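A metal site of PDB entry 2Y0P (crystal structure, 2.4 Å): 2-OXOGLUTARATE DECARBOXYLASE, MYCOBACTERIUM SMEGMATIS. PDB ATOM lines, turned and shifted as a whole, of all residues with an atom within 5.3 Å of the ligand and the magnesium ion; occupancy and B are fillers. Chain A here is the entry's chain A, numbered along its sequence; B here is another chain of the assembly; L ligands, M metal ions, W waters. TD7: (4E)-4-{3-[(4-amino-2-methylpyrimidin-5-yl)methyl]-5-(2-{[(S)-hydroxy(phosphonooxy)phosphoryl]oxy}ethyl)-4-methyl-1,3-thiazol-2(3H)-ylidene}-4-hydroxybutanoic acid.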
ATOM      1  N   PHE A 147     -16.859  -9.024 -18.248  1.00  0.00           N
ATOM      2  CA  PHE A 147     -16.803 -10.113 -17.244  1.00  0.00           C
ATOM      3  C   PHE A 147     -17.277 -11.434 -17.841  1.00  0.00           C
ATOM      4  O   PHE A 147     -18.350 -11.930 -17.501  1.00  0.00           O
ATOM      5  CB  PHE A 147     -17.577  -9.763 -15.968  1.00  0.00           C
ATOM      6  CG  PHE A 147     -16.946  -8.630 -15.212  1.00  0.00           C
ATOM      7  CD1 PHE A 147     -15.709  -8.781 -14.590  1.00  0.00           C
ATOM      8  CD2 PHE A 147     -17.574  -7.387 -15.143  1.00  0.00           C
ATOM      9  CE1 PHE A 147     -15.127  -7.720 -13.899  1.00  0.00           C
ATOM     10  CE2 PHE A 147     -16.991  -6.330 -14.439  1.00  0.00           C
ATOM     11  CZ  PHE A 147     -15.771  -6.506 -13.824  1.00  0.00           C
ATOM     12  N   HIS A 180     -21.887 -10.249 -11.863  1.00  0.00           N
ATOM     13  CA  HIS A 180     -21.287  -9.810 -13.115  1.00  0.00           C
ATOM     14  C   HIS A 180     -20.913 -10.957 -14.083  1.00  0.00           C
ATOM     15  O   HIS A 180     -21.036 -10.785 -15.286  1.00  0.00           O
ATOM     16  CB  HIS A 180     -20.021  -8.977 -12.798  1.00  0.00           C
ATOM     17  CG  HIS A 180     -19.038  -9.692 -11.904  1.00  0.00           C
ATOM     18  ND1 HIS A 180     -19.293  -9.892 -10.551  1.00  0.00           N
ATOM     19  CD2 HIS A 180     -17.842 -10.247 -12.202  1.00  0.00           C
ATOM     20  CE1 HIS A 180     -18.250 -10.572 -10.082  1.00  0.00           C
ATOM     21  NE2 HIS A 180     -17.353 -10.795 -11.042  1.00  0.00           N
ATOM     22  N   ARG A 181     -20.434 -12.105 -13.544  1.00  0.00           N
ATOM     23  CA  ARG A 181     -19.931 -13.255 -14.298  1.00  0.00           C
ATOM     24  C   ARG A 181     -20.985 -13.849 -15.259  1.00  0.00           C
ATOM     25  O   ARG A 181     -21.947 -14.481 -14.822  1.00  0.00           O
ATOM     26  CB  ARG A 181     -19.404 -14.338 -13.345  1.00  0.00           C
ATOM     27  CG  ARG A 181     -18.484 -15.396 -13.984  1.00  0.00           C
ATOM     28  CD  ARG A 181     -17.273 -14.832 -14.706  1.00  0.00           C
ATOM     29  NE  ARG A 181     -16.398 -14.061 -13.809  1.00  0.00           N
ATOM     30  CZ  ARG A 181     -15.460 -13.214 -14.219  1.00  0.00           C
ATOM     31  NH1 ARG A 181     -15.272 -13.005 -15.520  1.00  0.00           N
ATOM     32  NH2 ARG A 181     -14.713 -12.559 -13.345  1.00  0.00           N
ATOM     33  N   VAL A 217     -23.906   0.575 -15.269  1.00  0.00           N
ATOM     34  CA  VAL A 217     -23.126  -0.267 -16.170  1.00  0.00           C
ATOM     35  C   VAL A 217     -23.996  -1.443 -16.686  1.00  0.00           C
ATOM     36  O   VAL A 217     -24.926  -1.889 -15.988  1.00  0.00           O
ATOM     37  CB  VAL A 217     -21.790  -0.743 -15.519  1.00  0.00           C
ATOM     38  CG1 VAL A 217     -20.854   0.436 -15.238  1.00  0.00           C
ATOM     39  CG2 VAL A 217     -22.039  -1.538 -14.250  1.00  0.00           C
ATOM     40  N   TYR A 219     -23.579  -4.680 -17.112  1.00  0.00           N
ATOM     41  CA  TYR A 219     -23.606  -5.932 -16.358  1.00  0.00           C
ATOM     42  C   TYR A 219     -24.307  -5.786 -14.959  1.00  0.00           C
ATOM     43  O   TYR A 219     -24.069  -6.597 -14.063  1.00  0.00           O
ATOM     44  CB  TYR A 219     -22.179  -6.549 -16.222  1.00  0.00           C
ATOM     45  CG  TYR A 219     -21.111  -5.557 -15.809  1.00  0.00           C
ATOM     46  CD1 TYR A 219     -20.892  -5.250 -14.470  1.00  0.00           C
ATOM     47  CD2 TYR A 219     -20.321  -4.921 -16.764  1.00  0.00           C
ATOM     48  CE1 TYR A 219     -19.918  -4.331 -14.091  1.00  0.00           C
ATOM     49  CE2 TYR A 219     -19.335  -3.996 -16.390  1.00  0.00           C
ATOM     50  CZ  TYR A 219     -19.157  -3.698 -15.051  1.00  0.00           C
ATOM     51  OH  TYR A 219     -18.187  -2.792 -14.661  1.00  0.00           O
ATOM     52  N   HIS A 220     -25.198  -4.792 -14.806  1.00  0.00           N
ATOM     53  CA  HIS A 220     -25.999  -4.544 -13.598  1.00  0.00           C
ATOM     54  C   HIS A 220     -27.473  -4.475 -13.934  1.00  0.00           C
ATOM     55  O   HIS A 220     -28.315  -4.402 -13.042  1.00  0.00           O
ATOM     56  CB  HIS A 220     -25.603  -3.206 -12.946  1.00  0.00           C
ATOM     57  CG  HIS A 220     -24.339  -3.244 -12.161  1.00  0.00           C
ATOM     58  ND1 HIS A 220     -23.945  -2.161 -11.414  1.00  0.00           N
ATOM     59  CD2 HIS A 220     -23.412  -4.228 -12.031  1.00  0.00           C
ATOM     60  CE1 HIS A 220     -22.796  -2.509 -10.858  1.00  0.00           C
ATOM     61  NE2 HIS A 220     -22.440  -3.742 -11.197  1.00  0.00           N
ATOM     62  N   PRO A 244     -26.485  -3.575  -7.663  1.00  0.00           N
ATOM     63  CA  PRO A 244     -25.257  -2.785  -7.685  1.00  0.00           C
ATOM     64  C   PRO A 244     -24.012  -3.688  -7.825  1.00  0.00           C
ATOM     65  O   PRO A 244     -24.145  -4.903  -8.021  1.00  0.00           O
ATOM     66  CB  PRO A 244     -25.302  -2.050  -6.345  1.00  0.00           C
ATOM     67  CG  PRO A 244     -26.000  -3.011  -5.437  1.00  0.00           C
ATOM     68  CD  PRO A 244     -26.887  -3.879  -6.275  1.00  0.00           C
ATOM     69  N   SER A 245     -22.808  -3.100  -7.703  1.00  0.00           N
ATOM     70  CA  SER A 245     -21.549  -3.843  -7.769  1.00  0.00           C
ATOM     71  C   SER A 245     -21.394  -4.710  -6.542  1.00  0.00           C
ATOM     72  O   SER A 245     -20.833  -5.793  -6.636  1.00  0.00           O
ATOM     73  CB  SER A 245     -20.351  -2.910  -7.899  1.00  0.00           C
ATOM     74  OG  SER A 245     -20.218  -2.377  -9.202  1.00  0.00           O
ATOM     75  N   HIS A 246     -21.935  -4.230  -5.395  1.00  0.00           N
ATOM     76  CA  HIS A 246     -21.928  -4.872  -4.078  1.00  0.00           C
ATOM     77  C   HIS A 246     -22.431  -6.286  -4.218  1.00  0.00           C
ATOM     78  O   HIS A 246     -23.631  -6.564  -4.409  1.00  0.00           O
ATOM     79  CB  HIS A 246     -22.765  -4.054  -3.075  1.00  0.00           C
ATOM     80  CG  HIS A 246     -22.195  -2.699  -2.810  1.00  0.00           C
ATOM     81  ND1 HIS A 246     -22.003  -1.775  -3.839  1.00  0.00           N
ATOM     82  CD2 HIS A 246     -21.782  -2.143  -1.648  1.00  0.00           C
ATOM     83  CE1 HIS A 246     -21.463  -0.712  -3.272  1.00  0.00           C
ATOM     84  NE2 HIS A 246     -21.328  -0.874  -1.954  1.00  0.00           N
ATOM     85  N   LEU A 247     -21.461  -7.189  -4.220  1.00  0.00           N
ATOM     86  CA  LEU A 247     -21.678  -8.599  -4.407  1.00  0.00           C
ATOM     87  C   LEU A 247     -22.535  -9.162  -3.306  1.00  0.00           C
ATOM     88  O   LEU A 247     -22.327  -8.839  -2.132  1.00  0.00           O
ATOM     89  CB  LEU A 247     -20.334  -9.346  -4.502  1.00  0.00           C
ATOM     90  CG  LEU A 247     -19.513  -9.056  -5.766  1.00  0.00           C
ATOM     91  CD1 LEU A 247     -18.130  -9.632  -5.665  1.00  0.00           C
ATOM     92  CD2 LEU A 247     -20.216  -9.592  -7.007  1.00  0.00           C
ATOM     93  N   GLY A 285     -20.792 -15.940  -7.099  1.00  0.00           N
ATOM     94  CA  GLY A 285     -19.375 -16.193  -7.327  1.00  0.00           C
ATOM     95  C   GLY A 285     -18.851 -16.914  -6.100  1.00  0.00           C
ATOM     96  O   GLY A 285     -19.422 -16.766  -5.014  1.00  0.00           O
ATOM     97  N   ASP A 286     -17.782 -17.709  -6.251  1.00  0.00           N
ATOM     98  CA  ASP A 286     -17.237 -18.514  -5.150  1.00  0.00           C
ATOM     99  C   ASP A 286     -16.642 -17.681  -3.998  1.00  0.00           C
ATOM    100  O   ASP A 286     -16.774 -18.085  -2.839  1.00  0.00           O
ATOM    101  CB  ASP A 286     -16.194 -19.521  -5.660  1.00  0.00           C
ATOM    102  CG  ASP A 286     -15.040 -18.908  -6.452  1.00  0.00           C
ATOM    103  OD1 ASP A 286     -15.312 -18.197  -7.446  1.00  0.00           O
ATOM    104  OD2 ASP A 286     -13.876 -19.184  -6.104  1.00  0.00           O
ATOM    105  N   ALA A 287     -15.960 -16.562  -4.287  1.00  0.00           N
ATOM    106  CA  ALA A 287     -15.358 -15.748  -3.224  1.00  0.00           C
ATOM    107  C   ALA A 287     -16.420 -14.931  -2.484  1.00  0.00           C
ATOM    108  O   ALA A 287     -16.339 -14.796  -1.259  1.00  0.00           O
ATOM    109  CB  ALA A 287     -14.281 -14.831  -3.799  1.00  0.00           C
ATOM    110  N   ALA A 288     -17.426 -14.408  -3.223  1.00  0.00           N
ATOM    111  CA  ALA A 288     -18.487 -13.607  -2.659  1.00  0.00           C
ATOM    112  C   ALA A 288     -19.437 -14.441  -1.804  1.00  0.00           C
ATOM    113  O   ALA A 288     -19.893 -13.954  -0.772  1.00  0.00           O
ATOM    114  CB  ALA A 288     -19.239 -12.902  -3.765  1.00  0.00           C
ATOM    115  N   PHE A 289     -19.721 -15.702  -2.207  1.00  0.00           N
ATOM    116  CA  PHE A 289     -20.632 -16.596  -1.471  1.00  0.00           C
ATOM    117  C   PHE A 289     -20.085 -16.943  -0.085  1.00  0.00           C
ATOM    118  O   PHE A 289     -20.847 -16.963   0.876  1.00  0.00           O
ATOM    119  CB  PHE A 289     -20.911 -17.880  -2.262  1.00  0.00           C
ATOM    120  CG  PHE A 289     -22.149 -18.636  -1.833  1.00  0.00           C
ATOM    121  CD1 PHE A 289     -23.411 -18.099  -2.029  1.00  0.00           C
ATOM    122  CD2 PHE A 289     -22.049 -19.894  -1.261  1.00  0.00           C
ATOM    123  CE1 PHE A 289     -24.567 -18.818  -1.674  1.00  0.00           C
ATOM    124  CE2 PHE A 289     -23.198 -20.600  -0.880  1.00  0.00           C
ATOM    125  CZ  PHE A 289     -24.443 -20.059  -1.091  1.00  0.00           C
ATOM    126  N   GLN A 292     -19.329 -12.849   1.962  1.00  0.00           N
ATOM    127  CA  GLN A 292     -20.372 -11.866   2.286  1.00  0.00           C
ATOM    128  C   GLN A 292     -21.374 -12.400   3.303  1.00  0.00           C
ATOM    129  O   GLN A 292     -21.996 -13.444   3.075  1.00  0.00           O
ATOM    130  CB  GLN A 292     -21.081 -11.390   1.013  1.00  0.00           C
ATOM    131  CG  GLN A 292     -20.214 -10.476   0.137  1.00  0.00           C
ATOM    132  CD  GLN A 292     -19.991  -9.122   0.783  1.00  0.00           C
ATOM    133  OE1 GLN A 292     -20.937  -8.374   1.046  1.00  0.00           O
ATOM    134  NE2 GLN A 292     -18.738  -8.808   1.073  1.00  0.00           N
ATOM    135  N   VAL A 317     -21.062 -20.102  -9.521  1.00  0.00           N
ATOM    136  CA  VAL A 317     -20.118 -20.148 -10.642  1.00  0.00           C
ATOM    137  C   VAL A 317     -18.758 -20.149  -9.971  1.00  0.00           C
ATOM    138  O   VAL A 317     -18.169 -19.086  -9.721  1.00  0.00           O
ATOM    139  CB  VAL A 317     -20.327 -19.002 -11.669  1.00  0.00           C
ATOM    140  CG1 VAL A 317     -19.352 -19.118 -12.852  1.00  0.00           C
ATOM    141  CG2 VAL A 317     -21.776 -18.944 -12.167  1.00  0.00           C
ATOM    142  N   ASN A 319     -15.301 -20.612 -10.186  1.00  0.00           N
ATOM    143  CA  ASN A 319     -14.149 -20.594 -11.090  1.00  0.00           C
ATOM    144  C   ASN A 319     -12.832 -20.659 -10.303  1.00  0.00           C
ATOM    145  O   ASN A 319     -11.759 -20.420 -10.869  1.00  0.00           O
ATOM    146  CB  ASN A 319     -14.185 -19.369 -12.036  1.00  0.00           C
ATOM    147  CG  ASN A 319     -14.454 -18.032 -11.385  1.00  0.00           C
ATOM    148  OD1 ASN A 319     -14.231 -17.828 -10.192  1.00  0.00           O
ATOM    149  ND2 ASN A 319     -14.923 -17.089 -12.178  1.00  0.00           N
ATOM    150  N   GLN A 320     -12.904 -21.041  -9.015  1.00  0.00           N
ATOM    151  CA  GLN A 320     -11.791 -21.276  -8.084  1.00  0.00           C
ATOM    152  C   GLN A 320     -10.831 -20.077  -7.984  1.00  0.00           C
ATOM    153  O   GLN A 320      -9.631 -20.261  -7.787  1.00  0.00           O
ATOM    154  CB  GLN A 320     -11.034 -22.558  -8.494  1.00  0.00           C
ATOM    155  CG  GLN A 320     -11.943 -23.791  -8.519  1.00  0.00           C
ATOM    156  CD  GLN A 320     -11.275 -24.974  -9.138  1.00  0.00           C
ATOM    157  OE1 GLN A 320     -10.404 -25.611  -8.546  1.00  0.00           O
ATOM    158  NE2 GLN A 320     -11.682 -25.303 -10.352  1.00  0.00           N
ATOM    159  N   ILE A 321     -11.388 -18.853  -8.083  1.00  0.00           N
ATOM    160  CA  ILE A 321     -10.641 -17.592  -8.046  1.00  0.00           C
ATOM    161  C   ILE A 321     -11.586 -16.421  -7.696  1.00  0.00           C
ATOM    162  O   ILE A 321     -12.768 -16.472  -8.016  1.00  0.00           O
ATOM    163  CB  ILE A 321      -9.896 -17.366  -9.430  1.00  0.00           C
ATOM    164  CG1 ILE A 321      -8.833 -16.249  -9.356  1.00  0.00           C
ATOM    165  CG2 ILE A 321     -10.841 -17.169 -10.630  1.00  0.00           C
ATOM    166  CD1 ILE A 321      -7.591 -16.632  -8.698  1.00  0.00           C
ATOM    167  N   GLY A 322     -11.024 -15.408  -7.058  1.00  0.00           N
ATOM    168  CA  GLY A 322     -11.681 -14.144  -6.711  1.00  0.00           C
ATOM    169  C   GLY A 322     -10.721 -13.039  -7.098  1.00  0.00           C
ATOM    170  O   GLY A 322      -9.877 -12.655  -6.289  1.00  0.00           O
ATOM    171  N   PHE A 323     -10.788 -12.583  -8.368  1.00  0.00           N
ATOM    172  CA  PHE A 323      -9.893 -11.585  -8.979  1.00  0.00           C
ATOM    173  C   PHE A 323      -8.427 -12.155  -8.934  1.00  0.00           C
ATOM    174  O   PHE A 323      -8.110 -13.006  -9.756  1.00  0.00           O
ATOM    175  CB  PHE A 323     -10.040 -10.187  -8.324  1.00  0.00           C
ATOM    176  CG  PHE A 323      -9.527  -8.966  -9.075  1.00  0.00           C
ATOM    177  CD1 PHE A 323      -8.582  -9.106 -10.093  1.00  0.00           C
ATOM    178  CD2 PHE A 323      -9.916  -7.691  -8.706  1.00  0.00           C
ATOM    179  CE1 PHE A 323      -8.110  -7.988 -10.778  1.00  0.00           C
ATOM    180  CE2 PHE A 323      -9.420  -6.570  -9.377  1.00  0.00           C
ATOM    181  CZ  PHE A 323      -8.522  -6.722 -10.410  1.00  0.00           C
ATOM    182  N   ARG A 384     -11.931 -19.587 -14.992  1.00  0.00           N
ATOM    183  CA  ARG A 384     -12.066 -18.281 -15.643  1.00  0.00           C
ATOM    184  C   ARG A 384     -10.965 -18.218 -16.708  1.00  0.00           C
ATOM    185  O   ARG A 384      -9.799 -18.097 -16.365  1.00  0.00           O
ATOM    186  CB  ARG A 384     -11.953 -17.181 -14.573  1.00  0.00           C
ATOM    187  CG  ARG A 384     -12.309 -15.775 -15.035  1.00  0.00           C
ATOM    188  CD  ARG A 384     -11.722 -14.767 -14.079  1.00  0.00           C
ATOM    189  NE  ARG A 384     -10.257 -14.840 -14.072  1.00  0.00           N
ATOM    190  CZ  ARG A 384      -9.487 -14.430 -13.064  1.00  0.00           C
ATOM    191  NH1 ARG A 384     -10.032 -13.919 -11.973  1.00  0.00           N
ATOM    192  NH2 ARG A 384      -8.166 -14.553 -13.138  1.00  0.00           N
ATOM    193  N   HIS A 388      -9.561 -11.467 -14.502  1.00  0.00           N
ATOM    194  CA  HIS A 388     -10.781 -11.100 -13.787  1.00  0.00           C
ATOM    195  C   HIS A 388     -11.720 -10.333 -14.712  1.00  0.00           C
ATOM    196  O   HIS A 388     -12.893 -10.689 -14.834  1.00  0.00           O
ATOM    197  CB  HIS A 388     -10.423 -10.283 -12.543  1.00  0.00           C
ATOM    198  CG  HIS A 388     -11.587  -9.817 -11.740  1.00  0.00           C
ATOM    199  ND1 HIS A 388     -12.436 -10.721 -11.131  1.00  0.00           N
ATOM    200  CD2 HIS A 388     -11.980  -8.561 -11.429  1.00  0.00           C
ATOM    201  CE1 HIS A 388     -13.335  -9.986 -10.488  1.00  0.00           C
ATOM    202  NE2 HIS A 388     -13.092  -8.681 -10.635  1.00  0.00           N
ATOM    203  N   GLN B 542      -8.804  -6.424  -0.280  1.00  0.00           N
ATOM    204  CA  GLN B 542      -9.116  -7.251  -1.433  1.00  0.00           C
ATOM    205  C   GLN B 542      -8.095  -7.021  -2.558  1.00  0.00           C
ATOM    206  O   GLN B 542      -7.988  -5.907  -3.079  1.00  0.00           O
ATOM    207  CB  GLN B 542     -10.559  -7.000  -1.905  1.00  0.00           C
ATOM    208  CG  GLN B 542     -11.598  -7.728  -1.054  1.00  0.00           C
ATOM    209  CD  GLN B 542     -12.919  -7.010  -0.963  1.00  0.00           C
ATOM    210  OE1 GLN B 542     -13.306  -6.243  -1.849  1.00  0.00           O
ATOM    211  NE2 GLN B 542     -13.659  -7.280   0.108  1.00  0.00           N
ATOM    212  N   ASP B 543      -7.300  -8.075  -2.881  1.00  0.00           N
ATOM    213  CA  ASP B 543      -6.271  -8.094  -3.917  1.00  0.00           C
ATOM    214  C   ASP B 543      -5.165  -7.041  -3.636  1.00  0.00           C
ATOM    215  O   ASP B 543      -4.557  -6.520  -4.564  1.00  0.00           O
ATOM    216  CB  ASP B 543      -6.921  -7.872  -5.308  1.00  0.00           C
ATOM    217  CG  ASP B 543      -8.078  -8.828  -5.568  1.00  0.00           C
ATOM    218  OD1 ASP B 543      -7.813 -10.029  -5.778  1.00  0.00           O
ATOM    219  OD2 ASP B 543      -9.238  -8.365  -5.541  1.00  0.00           O
ATOM    220  N   LEU B 591     -13.544 -11.842   0.743  1.00  0.00           N
ATOM    221  CA  LEU B 591     -14.421 -10.868   0.106  1.00  0.00           C
ATOM    222  C   LEU B 591     -15.444 -10.375   1.125  1.00  0.00           C
ATOM    223  O   LEU B 591     -16.640 -10.628   1.016  1.00  0.00           O
ATOM    224  CB  LEU B 591     -15.096 -11.416  -1.163  1.00  0.00           C
ATOM    225  CG  LEU B 591     -15.207 -10.410  -2.317  1.00  0.00           C
ATOM    226  CD1 LEU B 591     -15.367 -11.128  -3.623  1.00  0.00           C
ATOM    227  CD2 LEU B 591     -16.337  -9.408  -2.100  1.00  0.00           C
ATOM    228  N   GLU B 593     -16.125  -6.802   3.983  1.00  0.00           N
ATOM    229  CA  GLU B 593     -15.828  -5.421   4.335  1.00  0.00           C
ATOM    230  C   GLU B 593     -16.060  -5.295   5.831  1.00  0.00           C
ATOM    231  O   GLU B 593     -15.123  -4.914   6.543  1.00  0.00           O
ATOM    232  CB  GLU B 593     -16.676  -4.433   3.522  1.00  0.00           C
ATOM    233  CG  GLU B 593     -16.217  -4.274   2.090  1.00  0.00           C
ATOM    234  CD  GLU B 593     -16.668  -5.318   1.083  1.00  0.00           C
ATOM    235  OE1 GLU B 593     -17.693  -6.001   1.322  1.00  0.00           O
ATOM    236  OE2 GLU B 593     -15.997  -5.436   0.032  1.00  0.00           O
ATOM    237  N   GLN B 617     -11.298  -2.260  -2.202  1.00  0.00           N
ATOM    238  CA  GLN B 617     -11.077  -2.487  -3.625  1.00  0.00           C
ATOM    239  C   GLN B 617     -11.332  -1.153  -4.334  1.00  0.00           C
ATOM    240  O   GLN B 617     -10.488  -0.673  -5.104  1.00  0.00           O
ATOM    241  CB  GLN B 617     -11.978  -3.610  -4.159  1.00  0.00           C
ATOM    242  CG  GLN B 617     -11.671  -4.035  -5.609  1.00  0.00           C
ATOM    243  CD  GLN B 617     -11.007  -5.384  -5.670  1.00  0.00           C
ATOM    244  OE1 GLN B 617     -11.643  -6.408  -5.934  1.00  0.00           O
ATOM    245  NE2 GLN B 617      -9.717  -5.427  -5.395  1.00  0.00           N
ATOM    246  N   PHE B 618     -12.486  -0.538  -3.997  1.00  0.00           N
ATOM    247  CA  PHE B 618     -12.997   0.780  -4.373  1.00  0.00           C
ATOM    248  C   PHE B 618     -13.666   1.314  -3.125  1.00  0.00           C
ATOM    249  O   PHE B 618     -14.272   0.528  -2.397  1.00  0.00           O
ATOM    250  CB  PHE B 618     -13.973   0.690  -5.562  1.00  0.00           C
ATOM    251  CG  PHE B 618     -13.342   0.416  -6.909  1.00  0.00           C
ATOM    252  CD1 PHE B 618     -13.058  -0.889  -7.303  1.00  0.00           C
ATOM    253  CD2 PHE B 618     -13.054   1.445  -7.790  1.00  0.00           C
ATOM    254  CE1 PHE B 618     -12.467  -1.149  -8.546  1.00  0.00           C
ATOM    255  CE2 PHE B 618     -12.487   1.190  -9.037  1.00  0.00           C
ATOM    256  CZ  PHE B 618     -12.196  -0.115  -9.403  1.00  0.00           C
ATOM    257  N   PHE B 621     -17.267   0.409  -1.561  1.00  0.00           N
ATOM    258  CA  PHE B 621     -17.631  -0.804  -0.824  1.00  0.00           C
ATOM    259  C   PHE B 621     -17.475  -0.665   0.688  1.00  0.00           C
ATOM    260  O   PHE B 621     -17.906  -1.571   1.418  1.00  0.00           O
ATOM    261  CB  PHE B 621     -16.794  -2.004  -1.332  1.00  0.00           C
ATOM    262  CG  PHE B 621     -16.947  -2.230  -2.813  1.00  0.00           C
ATOM    263  CD1 PHE B 621     -18.211  -2.476  -3.363  1.00  0.00           C
ATOM    264  CD2 PHE B 621     -15.862  -2.110  -3.673  1.00  0.00           C
ATOM    265  CE1 PHE B 621     -18.359  -2.631  -4.746  1.00  0.00           C
ATOM    266  CE2 PHE B 621     -16.015  -2.278  -5.045  1.00  0.00           C
ATOM    267  CZ  PHE B 621     -17.266  -2.526  -5.574  1.00  0.00           C
ATOM    268  N   HIS B 661     -17.927   2.538  -8.656  1.00  0.00           N
ATOM    269  CA  HIS B 661     -16.491   2.584  -8.906  1.00  0.00           C
ATOM    270  C   HIS B 661     -16.062   4.050  -9.027  1.00  0.00           C
ATOM    271  O   HIS B 661     -15.233   4.393  -9.864  1.00  0.00           O
ATOM    272  CB  HIS B 661     -16.145   1.771 -10.173  1.00  0.00           C
ATOM    273  CG  HIS B 661     -16.410   0.305 -10.032  1.00  0.00           C
ATOM    274  ND1 HIS B 661     -15.436  -0.561  -9.582  1.00  0.00           N
ATOM    275  CD2 HIS B 661     -17.550  -0.395 -10.247  1.00  0.00           C
ATOM    276  CE1 HIS B 661     -16.001  -1.755  -9.565  1.00  0.00           C
ATOM    277  NE2 HIS B 661     -17.274  -1.697  -9.939  1.00  0.00           N
HETATM  278  O1B TD7 L   1     -15.215 -12.607 -10.546  1.00  0.00           O
HETATM  279  PB  TD7 L   1     -15.800 -14.012 -10.044  1.00  0.00           P
HETATM  280  O3B TD7 L   1     -14.711 -15.017  -9.998  1.00  0.00           O
HETATM  281  O2B TD7 L   1     -16.955 -14.548 -11.032  1.00  0.00           O
HETATM  282  O3A TD7 L   1     -16.441 -13.822  -8.688  1.00  0.00           O
HETATM  283  PA  TD7 L   1     -16.002 -13.990  -7.153  1.00  0.00           P
HETATM  284  O1A TD7 L   1     -17.204 -13.928  -6.271  1.00  0.00           O
HETATM  285  O2A TD7 L   1     -15.259 -15.402  -6.972  1.00  0.00           O
HETATM  286  O7  TD7 L   1     -15.012 -12.774  -6.737  1.00  0.00           O
HETATM  287  C7  TD7 L   1     -15.032 -11.522  -7.413  1.00  0.00           C
HETATM  288  C6  TD7 L   1     -14.078 -10.488  -6.794  1.00  0.00           C
HETATM  289  C5  TD7 L   1     -14.674  -9.121  -7.029  1.00  0.00           C
HETATM  290  S1  TD7 L   1     -15.628  -8.702  -8.447  1.00  0.00           S
HETATM  291  C4  TD7 L   1     -14.670  -8.043  -6.228  1.00  0.00           C
HETATM  292  CM4 TD7 L   1     -13.934  -8.151  -4.925  1.00  0.00           C
HETATM  293  N3  TD7 L   1     -15.299  -6.974  -6.678  1.00  0.00           N
HETATM  294  C2  TD7 L   1     -15.833  -7.116  -7.853  1.00  0.00           C
HETATM  295  OL1 TD7 L   1     -16.187  -4.717  -8.675  1.00  0.00           O
HETATM  296  CLB TD7 L   1     -17.692  -6.569  -9.558  1.00  0.00           C
HETATM  297  CLC TD7 L   1     -18.917  -4.877 -10.831  1.00  0.00           C
HETATM  298  OL2 TD7 L   1     -18.713  -3.659 -10.974  1.00  0.00           O
HETATM  299  OL3 TD7 L   1     -20.063  -5.350 -10.650  1.00  0.00           O
HETATM  300  C7' TD7 L   1     -15.364  -5.704  -5.922  1.00  0.00           C
HETATM  301  C5' TD7 L   1     -16.350  -5.813  -4.774  1.00  0.00           C
HETATM  302  C6' TD7 L   1     -15.893  -5.803  -3.466  1.00  0.00           C
HETATM  303  N1' TD7 L   1     -16.772  -5.902  -2.457  1.00  0.00           N
HETATM  304  C2' TD7 L   1     -18.076  -5.998  -2.701  1.00  0.00           C
HETATM  305  CM2 TD7 L   1     -19.039  -6.098  -1.552  1.00  0.00           C
HETATM  306  N3' TD7 L   1     -18.563  -5.992  -3.935  1.00  0.00           N
HETATM  307  C4' TD7 L   1     -17.739  -5.918  -4.986  1.00  0.00           C
HETATM  308  C13 TD7 L   1     -17.730  -5.813 -10.880  1.00  0.00           C
HETATM  309  N4' TD7 L   1     -18.292  -5.893  -6.254  1.00  0.00           N
HETATM  310  C11 TD7 L   1     -16.556  -6.087  -8.691  1.00  0.00           C
HETATM  311 MG    MG M   1     -14.618 -16.643  -8.592  1.00  0.00          MG
HETATM  312  O   HOH W   1     -12.229 -13.460 -10.396  1.00  0.00           O
HETATM  313  O   HOH W   2     -16.821 -16.969  -9.457  1.00  0.00           O
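The backbone NH (N) of Ala 287 sits close to an oxygen (O2A) of the ligand (3.0 Å). The backbone NH (N) of Asp 286 lies close to an oxygen (O2A) of the ligand. A nitrogen (N4') of the ligand sits at hydrogen-bond distance from the backbone carbonyl oxygen (O) of Ser 245. An oxygen (O1B) of the ligand sits at hydrogen-bond distance from a ring nitrogen (NE2) of His 180 (2.8 Å). OL3 of the ligand is in hydrogen-bond range of NE2 of His 220, at 2.9 Å. The guanidinium group of Arg 181 lies within salt-bridge range of an oxygen (O1B) of the ligand (2.8 Å). An oxygen (O1A) of the ligand is in hydrogen-bond range of the backbone NH (N) of Ala 288, 3.1 Å away. N of Leu 247 sits at hydrogen-bond distance from N3' of the ligand, at 3.1 Å. A ring nitrogen (NE2) of His 661 of chain B lies within hydrogen-bond range of an oxygen (OL2) of the ligand, 2.6 Å away. The side-chain hydroxyl (OG) of Ser 245 lies within hydrogen-bond range of an oxygen (OL2) of the ligand, 2.7 Å away. NE2 of His 388 sits close to S1 of the ligand (3.3 Å). A nitrogen (N1') of the ligand sits at hydrogen-bond distance from the side-chain carboxylate of Glu 593 of chain B, 2.6 Å away.
O of Leu 591 of chain B is in hydrogen-bond range of NE2 of Gln 292, at 2.8 Å. OD2 of Asp 543 of chain B sits at hydrogen-bond distance from NE2 of Gln 617 of chain B (3.0 Å). The side-chain hydroxyl (OG) of Ser 245 sits close to a ring nitrogen (NE2) of His 220. The backbone carbonyl oxygen (O) of His 388 sits at hydrogen-bond distance from the guanidinium group (NH2) of Arg 181. NE2 of His 661 of chain B is in hydrogen-bond range of OG of Ser 245 (3.1 Å). OE2 of Glu 593 of chain B sits at hydrogen-bond distance from NE2 of Gln 542 of chain B (3.0 Å). OE1 of Glu 593 of chain B is in hydrogen-bond range of NE2 of Gln 292. The side-chain amide nitrogen (NE2) of Gln 617 of chain B lies within hydrogen-bond range of the backbone carbonyl oxygen (O) of Gln 542 of chain B (2.9 Å).
Residues that only touch the ligand: Phe 147, Tyr 219, His 246, Gly 285, Gln 292, Gly 322, Gln 542 of chain B, Leu 591 of chain B, Gln 617 of chain B and Phe 621 of chain B. Hydrophobic or aromatic side chains that line the ligand: Phe 147, His 180, Tyr 219, His 220, Leu 247, Ala 287, Ala 288, His 388, Leu 591 of chain B, Phe 621 of chain B and His 661 of chain B. Of the 32 residues printed, 23 come within 4 Å of the ligand. The nearest printed residue that does not touch the ligand is Phe 323 (4.2 Å).
The magnesium ion is bound by the backbone carbonyl oxygen (O) of Ile 321 (1.9 Å), the side-chain amide oxygen (OD1) of Asn 319 (2.0 Å), the side-chain carboxylate (OD1) of Asp 286 (2.1 Å), an oxygen (O2A) of the ligand (2.1 Å), an oxygen (O3B) of the ligand (2.2 Å) and water W2 (2.4 Å).
Water W2 lies within hydrogen-bond range of O of Val 317 (2.5 Å), O2B of the ligand (2.9 Å), ND2 of Asn 319 (3.3 Å) and N of Asp 286 (3.4 Å). Water W1 lies within hydrogen-bond range of the backbone NH of Phe 323 (2.6 Å), the guanidinium group of Arg 384 (2.7 Å), a ring nitrogen (ND1) of His 388 (2.8 Å) and an oxygen (O1B) of the ligand (3.1 Å).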
